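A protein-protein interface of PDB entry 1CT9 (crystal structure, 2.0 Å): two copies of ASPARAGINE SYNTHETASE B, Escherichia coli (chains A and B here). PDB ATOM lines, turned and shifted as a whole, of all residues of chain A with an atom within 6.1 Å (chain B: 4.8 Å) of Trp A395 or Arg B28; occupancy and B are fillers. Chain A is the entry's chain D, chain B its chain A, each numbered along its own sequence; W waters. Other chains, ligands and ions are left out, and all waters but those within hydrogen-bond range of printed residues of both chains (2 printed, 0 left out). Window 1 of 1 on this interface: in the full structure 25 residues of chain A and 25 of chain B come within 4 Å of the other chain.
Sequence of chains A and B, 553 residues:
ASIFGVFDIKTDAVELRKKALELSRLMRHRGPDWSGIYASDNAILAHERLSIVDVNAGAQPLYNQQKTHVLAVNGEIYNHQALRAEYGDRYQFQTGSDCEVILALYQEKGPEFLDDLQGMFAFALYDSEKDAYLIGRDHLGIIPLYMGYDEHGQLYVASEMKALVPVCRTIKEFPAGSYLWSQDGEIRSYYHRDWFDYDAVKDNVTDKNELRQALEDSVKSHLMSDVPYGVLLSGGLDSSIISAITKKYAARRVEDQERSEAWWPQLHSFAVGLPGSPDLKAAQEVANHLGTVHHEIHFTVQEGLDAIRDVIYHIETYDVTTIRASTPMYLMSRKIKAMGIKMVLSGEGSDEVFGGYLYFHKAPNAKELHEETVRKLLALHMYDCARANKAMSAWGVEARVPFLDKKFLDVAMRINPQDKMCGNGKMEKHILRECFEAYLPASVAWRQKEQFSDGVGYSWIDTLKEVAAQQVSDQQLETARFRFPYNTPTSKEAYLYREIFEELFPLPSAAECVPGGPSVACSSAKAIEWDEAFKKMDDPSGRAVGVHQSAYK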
ATOM      1  N   HIS A  29      16.072  16.201  25.026  1.00  0.00           N
ATOM      2  CA  HIS A  29      17.379  15.844  24.460  1.00  0.00           C
ATOM      3  C   HIS A  29      17.869  14.484  24.964  1.00  0.00           C
ATOM      4  O   HIS A  29      18.735  13.825  24.372  1.00  0.00           O
ATOM      5  CB  HIS A  29      18.432  16.832  24.942  1.00  0.00           C
ATOM      6  CG  HIS A  29      18.235  17.280  26.346  1.00  0.00           C
ATOM      7  ND1 HIS A  29      17.325  18.261  26.681  1.00  0.00           N
ATOM      8  CD2 HIS A  29      18.900  16.923  27.492  1.00  0.00           C
ATOM      9  CE1 HIS A  29      17.446  18.493  27.969  1.00  0.00           C
ATOM     10  NE2 HIS A  29      18.359  17.701  28.506  1.00  0.00           N
ATOM     11  N   ARG A  30      17.359  14.099  26.137  1.00  0.00           N
ATOM     12  CA  ARG A  30      17.740  12.852  26.732  1.00  0.00           C
ATOM     13  C   ARG A  30      17.067  11.693  25.986  1.00  0.00           C
ATOM     14  O   ARG A  30      17.556  10.554  25.985  1.00  0.00           O
ATOM     15  CB  ARG A  30      17.312  12.827  28.200  1.00  0.00           C
ATOM     16  CG  ARG A  30      17.915  13.896  29.083  1.00  0.00           C
ATOM     17  CD  ARG A  30      17.483  13.708  30.543  1.00  0.00           C
ATOM     18  NE  ARG A  30      17.838  12.375  31.038  1.00  0.00           N
ATOM     19  CZ  ARG A  30      18.968  12.101  31.706  1.00  0.00           C
ATOM     20  NH1 ARG A  30      19.873  13.051  31.973  1.00  0.00           N
ATOM     21  NH2 ARG A  30      19.230  10.837  32.090  1.00  0.00           N
ATOM     22  N   PRO A  32      15.492  11.549  22.370  1.00  0.00           N
ATOM     23  CA  PRO A  32      15.039  12.049  21.111  1.00  0.00           C
ATOM     24  C   PRO A  32      14.171  11.149  20.256  1.00  0.00           C
ATOM     25  O   PRO A  32      13.472  11.619  19.316  1.00  0.00           O
ATOM     26  CB  PRO A  32      16.306  12.481  20.372  1.00  0.00           C
ATOM     27  CG  PRO A  32      17.493  11.879  21.112  1.00  0.00           C
ATOM     28  CD  PRO A  32      16.962  11.264  22.368  1.00  0.00           C
ATOM     29  N   ASP A 310      25.162  26.547  27.904  1.00  0.00           N
ATOM     30  CA  ASP A 310      24.378  25.357  27.692  1.00  0.00           C
ATOM     31  C   ASP A 310      24.863  24.198  28.565  1.00  0.00           C
ATOM     32  O   ASP A 310      24.103  23.345  28.951  1.00  0.00           O
ATOM     33  CB  ASP A 310      24.397  24.944  26.215  1.00  0.00           C
ATOM     34  CG  ASP A 310      23.021  24.736  25.706  1.00  0.00           C
ATOM     35  OD1 ASP A 310      22.783  24.470  24.552  1.00  0.00           O
ATOM     36  OD2 ASP A 310      22.115  24.857  26.646  1.00  0.00           O
ATOM     37  N   HIS A 314      22.628  22.074  31.112  1.00  0.00           N
ATOM     38  CA  HIS A 314      22.589  20.622  31.085  1.00  0.00           C
ATOM     39  C   HIS A 314      23.010  19.862  32.320  1.00  0.00           C
ATOM     40  O   HIS A 314      22.395  18.885  32.736  1.00  0.00           O
ATOM     41  CB  HIS A 314      23.321  20.085  29.857  1.00  0.00           C
ATOM     42  CG  HIS A 314      22.443  20.290  28.707  1.00  0.00           C
ATOM     43  ND1 HIS A 314      21.419  19.367  28.406  1.00  0.00           N
ATOM     44  CD2 HIS A 314      22.384  21.312  27.805  1.00  0.00           C
ATOM     45  CE1 HIS A 314      20.780  19.835  27.320  1.00  0.00           C
ATOM     46  NE2 HIS A 314      21.318  21.000  26.936  1.00  0.00           N
ATOM     47  N   MET A 329      33.311  17.155  27.330  1.00  0.00           N
ATOM     48  CA  MET A 329      32.458  15.963  27.261  1.00  0.00           C
ATOM     49  C   MET A 329      31.147  16.224  26.553  1.00  0.00           C
ATOM     50  O   MET A 329      30.610  15.437  25.779  1.00  0.00           O
ATOM     51  CB  MET A 329      32.257  15.437  28.673  1.00  0.00           C
ATOM     52  CG  MET A 329      31.262  14.298  28.730  1.00  0.00           C
ATOM     53  SD  MET A 329      31.169  13.584  30.387  1.00  0.00           S
ATOM     54  CE  MET A 329      31.606  11.871  30.049  1.00  0.00           C
ATOM     55  N   TYR A 330      30.676  17.417  26.795  1.00  0.00           N
ATOM     56  CA  TYR A 330      29.486  17.905  26.204  1.00  0.00           C
ATOM     57  C   TYR A 330      29.681  18.054  24.703  1.00  0.00           C
ATOM     58  O   TYR A 330      28.843  17.690  23.873  1.00  0.00           O
ATOM     59  CB  TYR A 330      29.113  19.222  26.946  1.00  0.00           C
ATOM     60  CG  TYR A 330      28.022  20.024  26.241  1.00  0.00           C
ATOM     61  CD1 TYR A 330      28.401  20.928  25.249  1.00  0.00           C
ATOM     62  CD2 TYR A 330      26.655  19.897  26.492  1.00  0.00           C
ATOM     63  CE1 TYR A 330      27.480  21.686  24.528  1.00  0.00           C
ATOM     64  CE2 TYR A 330      25.712  20.629  25.763  1.00  0.00           C
ATOM     65  CZ  TYR A 330      26.119  21.554  24.800  1.00  0.00           C
ATOM     66  OH  TYR A 330      25.200  22.255  24.067  1.00  0.00           O
ATOM     67  N   LEU A 331      30.823  18.578  24.296  1.00  0.00           N
ATOM     68  CA  LEU A 331      31.005  18.721  22.834  1.00  0.00           C
ATOM     69  C   LEU A 331      31.326  17.369  22.163  1.00  0.00           C
ATOM     70  O   LEU A 331      31.015  17.089  21.005  1.00  0.00           O
ATOM     71  CB  LEU A 331      32.107  19.780  22.537  1.00  0.00           C
ATOM     72  CG  LEU A 331      31.895  21.198  23.123  1.00  0.00           C
ATOM     73  CD1 LEU A 331      33.212  21.967  23.211  1.00  0.00           C
ATOM     74  CD2 LEU A 331      31.019  21.952  22.148  1.00  0.00           C
ATOM     75  N   SER A 333      30.180  14.617  22.990  1.00  0.00           N
ATOM     76  CA  SER A 333      28.875  13.990  22.831  1.00  0.00           C
ATOM     77  C   SER A 333      28.122  14.432  21.575  1.00  0.00           C
ATOM     78  O   SER A 333      27.488  13.637  20.799  1.00  0.00           O
ATOM     79  CB  SER A 333      28.102  14.249  24.162  1.00  0.00           C
ATOM     80  OG  SER A 333      26.796  13.644  24.122  1.00  0.00           O
ATOM     81  N   ARG A 334      28.134  15.746  21.313  1.00  0.00           N
ATOM     82  CA  ARG A 334      27.434  16.175  20.121  1.00  0.00           C
ATOM     83  C   ARG A 334      27.980  15.549  18.827  1.00  0.00           C
ATOM     84  O   ARG A 334      27.198  15.203  17.910  1.00  0.00           O
ATOM     85  CB  ARG A 334      27.459  17.686  20.045  1.00  0.00           C
ATOM     86  CG  ARG A 334      26.919  18.181  18.725  1.00  0.00           C
ATOM     87  CD  ARG A 334      26.826  19.706  18.793  1.00  0.00           C
ATOM     88  NE  ARG A 334      25.851  20.249  17.863  1.00  0.00           N
ATOM     89  CZ  ARG A 334      25.589  21.541  17.795  1.00  0.00           C
ATOM     90  NH1 ARG A 334      26.206  22.387  18.622  1.00  0.00           N
ATOM     91  NH2 ARG A 334      24.671  21.955  16.917  1.00  0.00           N
ATOM     92  N   LYS A 335      29.334  15.424  18.792  1.00  0.00           N
ATOM     93  CA  LYS A 335      30.165  14.840  17.736  1.00  0.00           C
ATOM     94  C   LYS A 335      29.857  13.339  17.620  1.00  0.00           C
ATOM     95  O   LYS A 335      29.510  12.814  16.572  1.00  0.00           O
ATOM     96  CB  LYS A 335      31.625  15.198  18.058  1.00  0.00           C
ATOM     97  CG  LYS A 335      32.377  15.858  16.910  1.00  0.00           C
ATOM     98  CD  LYS A 335      32.369  17.382  16.828  1.00  0.00           C
ATOM     99  CE  LYS A 335      32.935  17.925  15.497  1.00  0.00           C
ATOM    100  NZ  LYS A 335      34.175  18.714  15.637  1.00  0.00           N
ATOM    101  N   LYS A 337      27.105  11.661  18.666  1.00  0.00           N
ATOM    102  CA  LYS A 337      25.746  11.490  18.210  1.00  0.00           C
ATOM    103  C   LYS A 337      25.570  11.722  16.748  1.00  0.00           C
ATOM    104  O   LYS A 337      24.805  11.069  16.100  1.00  0.00           O
ATOM    105  CB  LYS A 337      24.748  12.298  19.022  1.00  0.00           C
ATOM    106  CG  LYS A 337      23.351  12.044  18.473  1.00  0.00           C
ATOM    107  CD  LYS A 337      22.918  10.581  18.381  1.00  0.00           C
ATOM    108  CE  LYS A 337      22.249  10.054  19.644  1.00  0.00           C
ATOM    109  NZ  LYS A 337      20.782  10.186  19.645  1.00  0.00           N
ATOM    110  N   LYS A 390      24.627  13.583  32.437  1.00  0.00           N
ATOM    111  CA  LYS A 390      24.050  14.759  31.832  1.00  0.00           C
ATOM    112  C   LYS A 390      24.838  15.324  30.635  1.00  0.00           C
ATOM    113  O   LYS A 390      24.239  15.727  29.635  1.00  0.00           O
ATOM    114  CB  LYS A 390      23.842  15.785  32.910  1.00  0.00           C
ATOM    115  CG  LYS A 390      22.914  15.250  33.976  1.00  0.00           C
ATOM    116  CD  LYS A 390      22.966  16.085  35.228  1.00  0.00           C
ATOM    117  CE  LYS A 390      21.653  16.754  35.535  1.00  0.00           C
ATOM    118  NZ  LYS A 390      21.650  17.167  36.954  1.00  0.00           N
ATOM    119  N   ALA A 391      26.170  15.335  30.732  1.00  0.00           N
ATOM    120  CA  ALA A 391      26.999  15.775  29.620  1.00  0.00           C
ATOM    121  C   ALA A 391      26.632  14.957  28.396  1.00  0.00           C
ATOM    122  O   ALA A 391      26.379  15.520  27.288  1.00  0.00           O
ATOM    123  CB  ALA A 391      28.526  15.677  29.925  1.00  0.00           C
ATOM    124  N   MET A 392      26.612  13.624  28.576  1.00  0.00           N
ATOM    125  CA  MET A 392      26.309  12.765  27.430  1.00  0.00           C
ATOM    126  C   MET A 392      24.862  12.857  26.927  1.00  0.00           C
ATOM    127  O   MET A 392      24.577  12.915  25.691  1.00  0.00           O
ATOM    128  CB  MET A 392      26.826  11.304  27.516  1.00  0.00           C
ATOM    129  CG  MET A 392      28.268  11.174  27.957  1.00  0.00           C
ATOM    130  SD  MET A 392      29.455  11.851  26.785  1.00  0.00           S
ATOM    131  CE  MET A 392      28.792  11.194  25.252  1.00  0.00           C
ATOM    132  N   SER A 393      23.924  12.901  27.881  1.00  0.00           N
ATOM    133  CA  SER A 393      22.489  12.988  27.576  1.00  0.00           C
ATOM    134  C   SER A 393      22.047  14.272  26.896  1.00  0.00           C
ATOM    135  O   SER A 393      20.953  14.326  26.315  1.00  0.00           O
ATOM    136  CB  SER A 393      21.632  12.765  28.806  1.00  0.00           C
ATOM    137  OG  SER A 393      21.809  11.450  29.296  1.00  0.00           O
ATOM    138  N   ALA A 394      22.919  15.279  26.958  1.00  0.00           N
ATOM    139  CA  ALA A 394      22.647  16.576  26.355  1.00  0.00           C
ATOM    140  C   ALA A 394      22.408  16.401  24.900  1.00  0.00           C
ATOM    141  O   ALA A 394      21.698  17.195  24.270  1.00  0.00           O
ATOM    142  CB  ALA A 394      23.833  17.546  26.542  1.00  0.00           C
ATOM    143  N   TRP A 395      23.050  15.334  24.397  1.00  0.00           N
ATOM    144  CA  TRP A 395      22.963  14.991  22.999  1.00  0.00           C
ATOM    145  C   TRP A 395      22.349  13.650  22.739  1.00  0.00           C
ATOM    146  O   TRP A 395      22.477  13.202  21.636  1.00  0.00           O
ATOM    147  CB  TRP A 395      24.261  15.203  22.179  1.00  0.00           C
ATOM    148  CG  TRP A 395      24.778  16.607  22.349  1.00  0.00           C
ATOM    149  CD1 TRP A 395      25.667  17.075  23.273  1.00  0.00           C
ATOM    150  CD2 TRP A 395      24.336  17.754  21.600  1.00  0.00           C
ATOM    151  NE1 TRP A 395      25.827  18.432  23.152  1.00  0.00           N
ATOM    152  CE2 TRP A 395      25.006  18.874  22.144  1.00  0.00           C
ATOM    153  CE3 TRP A 395      23.413  17.918  20.549  1.00  0.00           C
ATOM    154  CZ2 TRP A 395      24.761  20.160  21.661  1.00  0.00           C
ATOM    155  CZ3 TRP A 395      23.160  19.187  20.092  1.00  0.00           C
ATOM    156  CH2 TRP A 395      23.835  20.279  20.646  1.00  0.00           C
ATOM    157  N   GLY A 396      21.673  13.031  23.705  1.00  0.00           N
ATOM    158  CA  GLY A 396      21.016  11.739  23.455  1.00  0.00           C
ATOM    159  C   GLY A 396      22.009  10.592  23.326  1.00  0.00           C
ATOM    160  O   GLY A 396      21.951   9.783  22.412  1.00  0.00           O
ATOM    161  N   VAL A 397      22.967  10.576  24.219  1.00  0.00           N
ATOM    162  CA  VAL A 397      23.992   9.562  24.206  1.00  0.00           C
ATOM    163  C   VAL A 397      24.081   8.972  25.568  1.00  0.00           C
ATOM    164  O   VAL A 397      24.278   9.681  26.572  1.00  0.00           O
ATOM    165  CB  VAL A 397      25.376  10.124  23.801  1.00  0.00           C
ATOM    166  CG1 VAL A 397      26.444   9.028  23.923  1.00  0.00           C
ATOM    167  CG2 VAL A 397      25.346  10.534  22.327  1.00  0.00           C
ATOM    168  N   SER B  24      20.393  31.812  17.915  1.00  0.00           N
ATOM    169  CA  SER B  24      20.771  30.753  16.999  1.00  0.00           C
ATOM    170  C   SER B  24      20.408  29.381  17.637  1.00  0.00           C
ATOM    171  O   SER B  24      19.862  28.470  17.022  1.00  0.00           O
ATOM    172  CB  SER B  24      22.243  30.855  16.571  1.00  0.00           C
ATOM    173  OG  SER B  24      22.642  29.726  15.787  1.00  0.00           O
ATOM    174  N   ARG B  25      20.694  29.218  18.929  1.00  0.00           N
ATOM    175  CA  ARG B  25      20.361  28.019  19.625  1.00  0.00           C
ATOM    176  C   ARG B  25      18.884  27.602  19.514  1.00  0.00           C
ATOM    177  O   ARG B  25      18.524  26.418  19.459  1.00  0.00           O
ATOM    178  CB  ARG B  25      20.842  28.103  21.041  1.00  0.00           C
ATOM    179  CG  ARG B  25      20.189  27.043  21.906  1.00  0.00           C
ATOM    180  CD  ARG B  25      20.722  27.109  23.354  1.00  0.00           C
ATOM    181  NE  ARG B  25      19.983  26.322  24.361  1.00  0.00           N
ATOM    182  CZ  ARG B  25      18.648  26.247  24.497  1.00  0.00           C
ATOM    183  NH1 ARG B  25      17.805  26.893  23.687  1.00  0.00           N
ATOM    184  NH2 ARG B  25      18.136  25.503  25.475  1.00  0.00           N
ATOM    185  N   LEU B  26      17.972  28.554  19.430  1.00  0.00           N
ATOM    186  CA  LEU B  26      16.571  28.192  19.324  1.00  0.00           C
ATOM    187  C   LEU B  26      16.290  27.389  18.080  1.00  0.00           C
ATOM    188  O   LEU B  26      15.217  26.831  17.964  1.00  0.00           O
ATOM    189  CB  LEU B  26      15.638  29.409  19.245  1.00  0.00           C
ATOM    190  CG  LEU B  26      15.794  30.282  20.467  1.00  0.00           C
ATOM    191  CD1 LEU B  26      14.857  31.486  20.293  1.00  0.00           C
ATOM    192  CD2 LEU B  26      15.422  29.453  21.695  1.00  0.00           C
ATOM    193  N   MET B  27      17.214  27.345  17.115  1.00  0.00           N
ATOM    194  CA  MET B  27      16.907  26.586  15.900  1.00  0.00           C
ATOM    195  C   MET B  27      17.814  25.344  15.773  1.00  0.00           C
ATOM    196  O   MET B  27      17.897  24.694  14.734  1.00  0.00           O
ATOM    197  CB  MET B  27      17.074  27.480  14.638  1.00  0.00           C
ATOM    198  CG  MET B  27      16.321  28.798  14.663  1.00  0.00           C
ATOM    199  SD  MET B  27      16.750  29.816  13.212  1.00  0.00           S
ATOM    200  CE  MET B  27      18.347  30.516  13.782  1.00  0.00           C
ATOM    201  N   ARG B  28      18.527  25.033  16.842  1.00  0.00           N
ATOM    202  CA  ARG B  28      19.460  23.932  16.805  1.00  0.00           C
ATOM    203  C   ARG B  28      18.953  22.595  16.261  1.00  0.00           C
ATOM    204  O   ARG B  28      19.714  21.765  15.788  1.00  0.00           O
ATOM    205  CB  ARG B  28      19.969  23.764  18.191  1.00  0.00           C
ATOM    206  CG  ARG B  28      21.203  22.898  18.226  1.00  0.00           C
ATOM    207  CD  ARG B  28      21.794  23.048  19.608  1.00  0.00           C
ATOM    208  NE  ARG B  28      22.473  24.305  19.762  1.00  0.00           N
ATOM    209  CZ  ARG B  28      23.028  24.645  20.919  1.00  0.00           C
ATOM    210  NH1 ARG B  28      22.929  23.855  21.966  1.00  0.00           N
ATOM    211  NH2 ARG B  28      23.614  25.841  21.025  1.00  0.00           N
ATOM    212  N   HIS B  29      17.660  22.363  16.395  1.00  0.00           N
ATOM    213  CA  HIS B  29      17.044  21.140  15.905  1.00  0.00           C
ATOM    214  C   HIS B  29      17.356  20.993  14.426  1.00  0.00           C
ATOM    215  O   HIS B  29      17.398  19.896  13.888  1.00  0.00           O
ATOM    216  CB  HIS B  29      15.501  21.161  16.133  1.00  0.00           C
ATOM    217  CG  HIS B  29      14.830  22.483  15.741  1.00  0.00           C
ATOM    218  ND1 HIS B  29      14.774  23.577  16.615  1.00  0.00           N
ATOM    219  CD2 HIS B  29      14.238  22.884  14.576  1.00  0.00           C
ATOM    220  CE1 HIS B  29      14.120  24.551  16.007  1.00  0.00           C
ATOM    221  NE2 HIS B  29      13.778  24.164  14.785  1.00  0.00           N
ATOM    222  N   ARG B  30      17.508  22.112  13.742  1.00  0.00           N
ATOM    223  CA  ARG B  30      17.755  21.999  12.347  1.00  0.00           C
ATOM    224  C   ARG B  30      19.211  21.626  12.040  1.00  0.00           C
ATOM    225  O   ARG B  30      19.451  21.125  10.937  1.00  0.00           O
ATOM    226  CB  ARG B  30      17.367  23.187  11.461  1.00  0.00           C
ATOM    227  CG  ARG B  30      16.232  24.079  11.894  1.00  0.00           C
ATOM    228  CD  ARG B  30      16.116  25.359  11.046  1.00  0.00           C
ATOM    229  NE  ARG B  30      16.265  25.220   9.586  1.00  0.00           N
ATOM    230  CZ  ARG B  30      15.276  24.880   8.763  1.00  0.00           C
ATOM    231  NH1 ARG B  30      14.066  24.608   9.207  1.00  0.00           N
ATOM    232  NH2 ARG B  30      15.468  24.804   7.455  1.00  0.00           N
ATOM    233  N   GLY B  31      20.147  21.889  12.960  1.00  0.00           N
ATOM    234  CA  GLY B  31      21.552  21.567  12.703  1.00  0.00           C
ATOM    235  C   GLY B  31      22.194  21.055  13.960  1.00  0.00           C
ATOM    236  O   GLY B  31      23.039  21.651  14.606  1.00  0.00           O
ATOM    237  N   PRO B  32      21.755  19.884  14.353  1.00  0.00           N
ATOM    238  CA  PRO B  32      22.224  19.278  15.578  1.00  0.00           C
ATOM    239  C   PRO B  32      23.679  18.898  15.631  1.00  0.00           C
ATOM    240  O   PRO B  32      24.218  18.719  16.724  1.00  0.00           O
ATOM    241  CB  PRO B  32      21.473  17.939  15.682  1.00  0.00           C
ATOM    242  CG  PRO B  32      20.753  17.713  14.351  1.00  0.00           C
ATOM    243  CD  PRO B  32      20.793  19.049  13.608  1.00  0.00           C
ATOM    244  N   SER B  35      27.962  23.585  15.633  1.00  0.00           N
ATOM    245  CA  SER B  35      27.668  24.974  15.610  1.00  0.00           C
ATOM    246  C   SER B  35      28.866  25.755  15.153  1.00  0.00           C
ATOM    247  O   SER B  35      29.984  25.421  15.514  1.00  0.00           O
ATOM    248  CB  SER B  35      27.554  25.379  17.077  1.00  0.00           C
ATOM    249  OG  SER B  35      26.197  25.481  17.494  1.00  0.00           O
ATOM    250  N   GLU B  48      24.085  26.443  12.474  1.00  0.00           N
ATOM    251  CA  GLU B  48      23.901  25.202  13.205  1.00  0.00           C
ATOM    252  C   GLU B  48      23.833  24.198  12.071  1.00  0.00           C
ATOM    253  O   GLU B  48      23.034  24.319  11.118  1.00  0.00           O
ATOM    254  CB  GLU B  48      22.655  25.118  14.110  1.00  0.00           C
ATOM    255  CG  GLU B  48      22.449  26.305  15.086  1.00  0.00           C
ATOM    256  CD  GLU B  48      23.270  26.188  16.351  1.00  0.00           C
ATOM    257  OE1 GLU B  48      23.666  27.131  17.048  1.00  0.00           O
ATOM    258  OE2 GLU B  48      23.527  24.942  16.624  1.00  0.00           O
HETATM  259  O   HOH W   1      19.856  22.556  25.146  1.00  0.00           O
HETATM  260  O   HOH W   2      24.692  15.802  17.570  1.00  0.00           O
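The guanidinium group (NH2) of Arg A334 is in salt-bridge range of the side-chain carboxylate (OE2) of Glu B48 (3.2 Å). NH1 of Arg B28 is in salt-bridge range of OD1 of Asp A310, 2.7 Å away. O of Gly B31 is in hydrogen-bond range of NH2 of Arg A334, at 2.8 Å. The guanidinium group of Arg A334 sits at hydrogen-bond distance from the side-chain hydroxyl of Ser B35 (3.3 Å). The guanidinium group (NH1) of Arg B28 is in hydrogen-bond range of the side-chain hydroxyl (OH) of Tyr A330 (3.5 Å). The side-chain carboxylate (OD1) of Asp A310 is in salt-bridge range of the guanidinium group (NE) of Arg B25. The backbone carbonyl oxygen of Pro B32 is in hydrogen-bond range of the guanidinium group of Arg A334, 2.5 Å away.
NE of Arg B28 is in salt-bridge range of OE2 of Glu B48, 3.4 Å away. OG of Ser B35 sits at hydrogen-bond distance from OE2 of Glu B48 (2.9 Å). OH of Tyr A330 sits at hydrogen-bond distance from OD1 of Asp A310, at 3.3 Å. O of Tyr A330 lies within hydrogen-bond range of NE1 of Trp A395. The side-chain hydroxyl of Ser B24 is in hydrogen-bond range of the side-chain carboxylate of Glu B48.
Among the printed residues, pairs that only touch across the chains: Trp A395 with Pro B32 (3.6 Å), Trp A395 with Arg B28 (3.6 Å) and Arg A334 with Arg B28 (3.8 Å).
Trp A395 touches two residues of chain B. Of chain A, only Asp A310 (2.7 Å), Tyr A330 (3.5 Å), Arg A334 (3.8 Å) and Trp A395 (3.6 Å) come within 4 Å of Arg B28. Of the printed residues of chain A, Gly B31 touches Arg A334 (2.8 Å). Of the printed residues of chain A, Pro B32 touches Arg A334 and Trp A395. Of the printed residues of chain A, Arg B25 touches Asp A310. The nearest residue of chain A that does not touch Arg B28 is His A314 (6.0 Å). The nearest printed residue of chain B that does not touch Arg A334 is His B29 (7.0 Å).
Of the 11 printed residues of chain B, 6 touch a printed residue of chain A. Printed residues of chain B that touch a printed residue of chain A: Arg B25, Arg B28, Gly B31, Pro B32, Ser B35 and Glu B48. Hydrophobic or aromatic side chains of chain A that line the printed part of chain B: Tyr A330 and Trp A395.
Positions printed for both chains: 29, 30 and 32.
Water W2 lies within hydrogen-bond range of the backbone carbonyl oxygen (O) of Arg A334 (2.6 Å) and the backbone carbonyl oxygen (O) of Pro B32 (3.1 Å). Water W1 bridges a ring nitrogen (NE2) of His A314 (2.8 Å) and the guanidinium group (NH2) of Arg B25 (3.4 Å).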
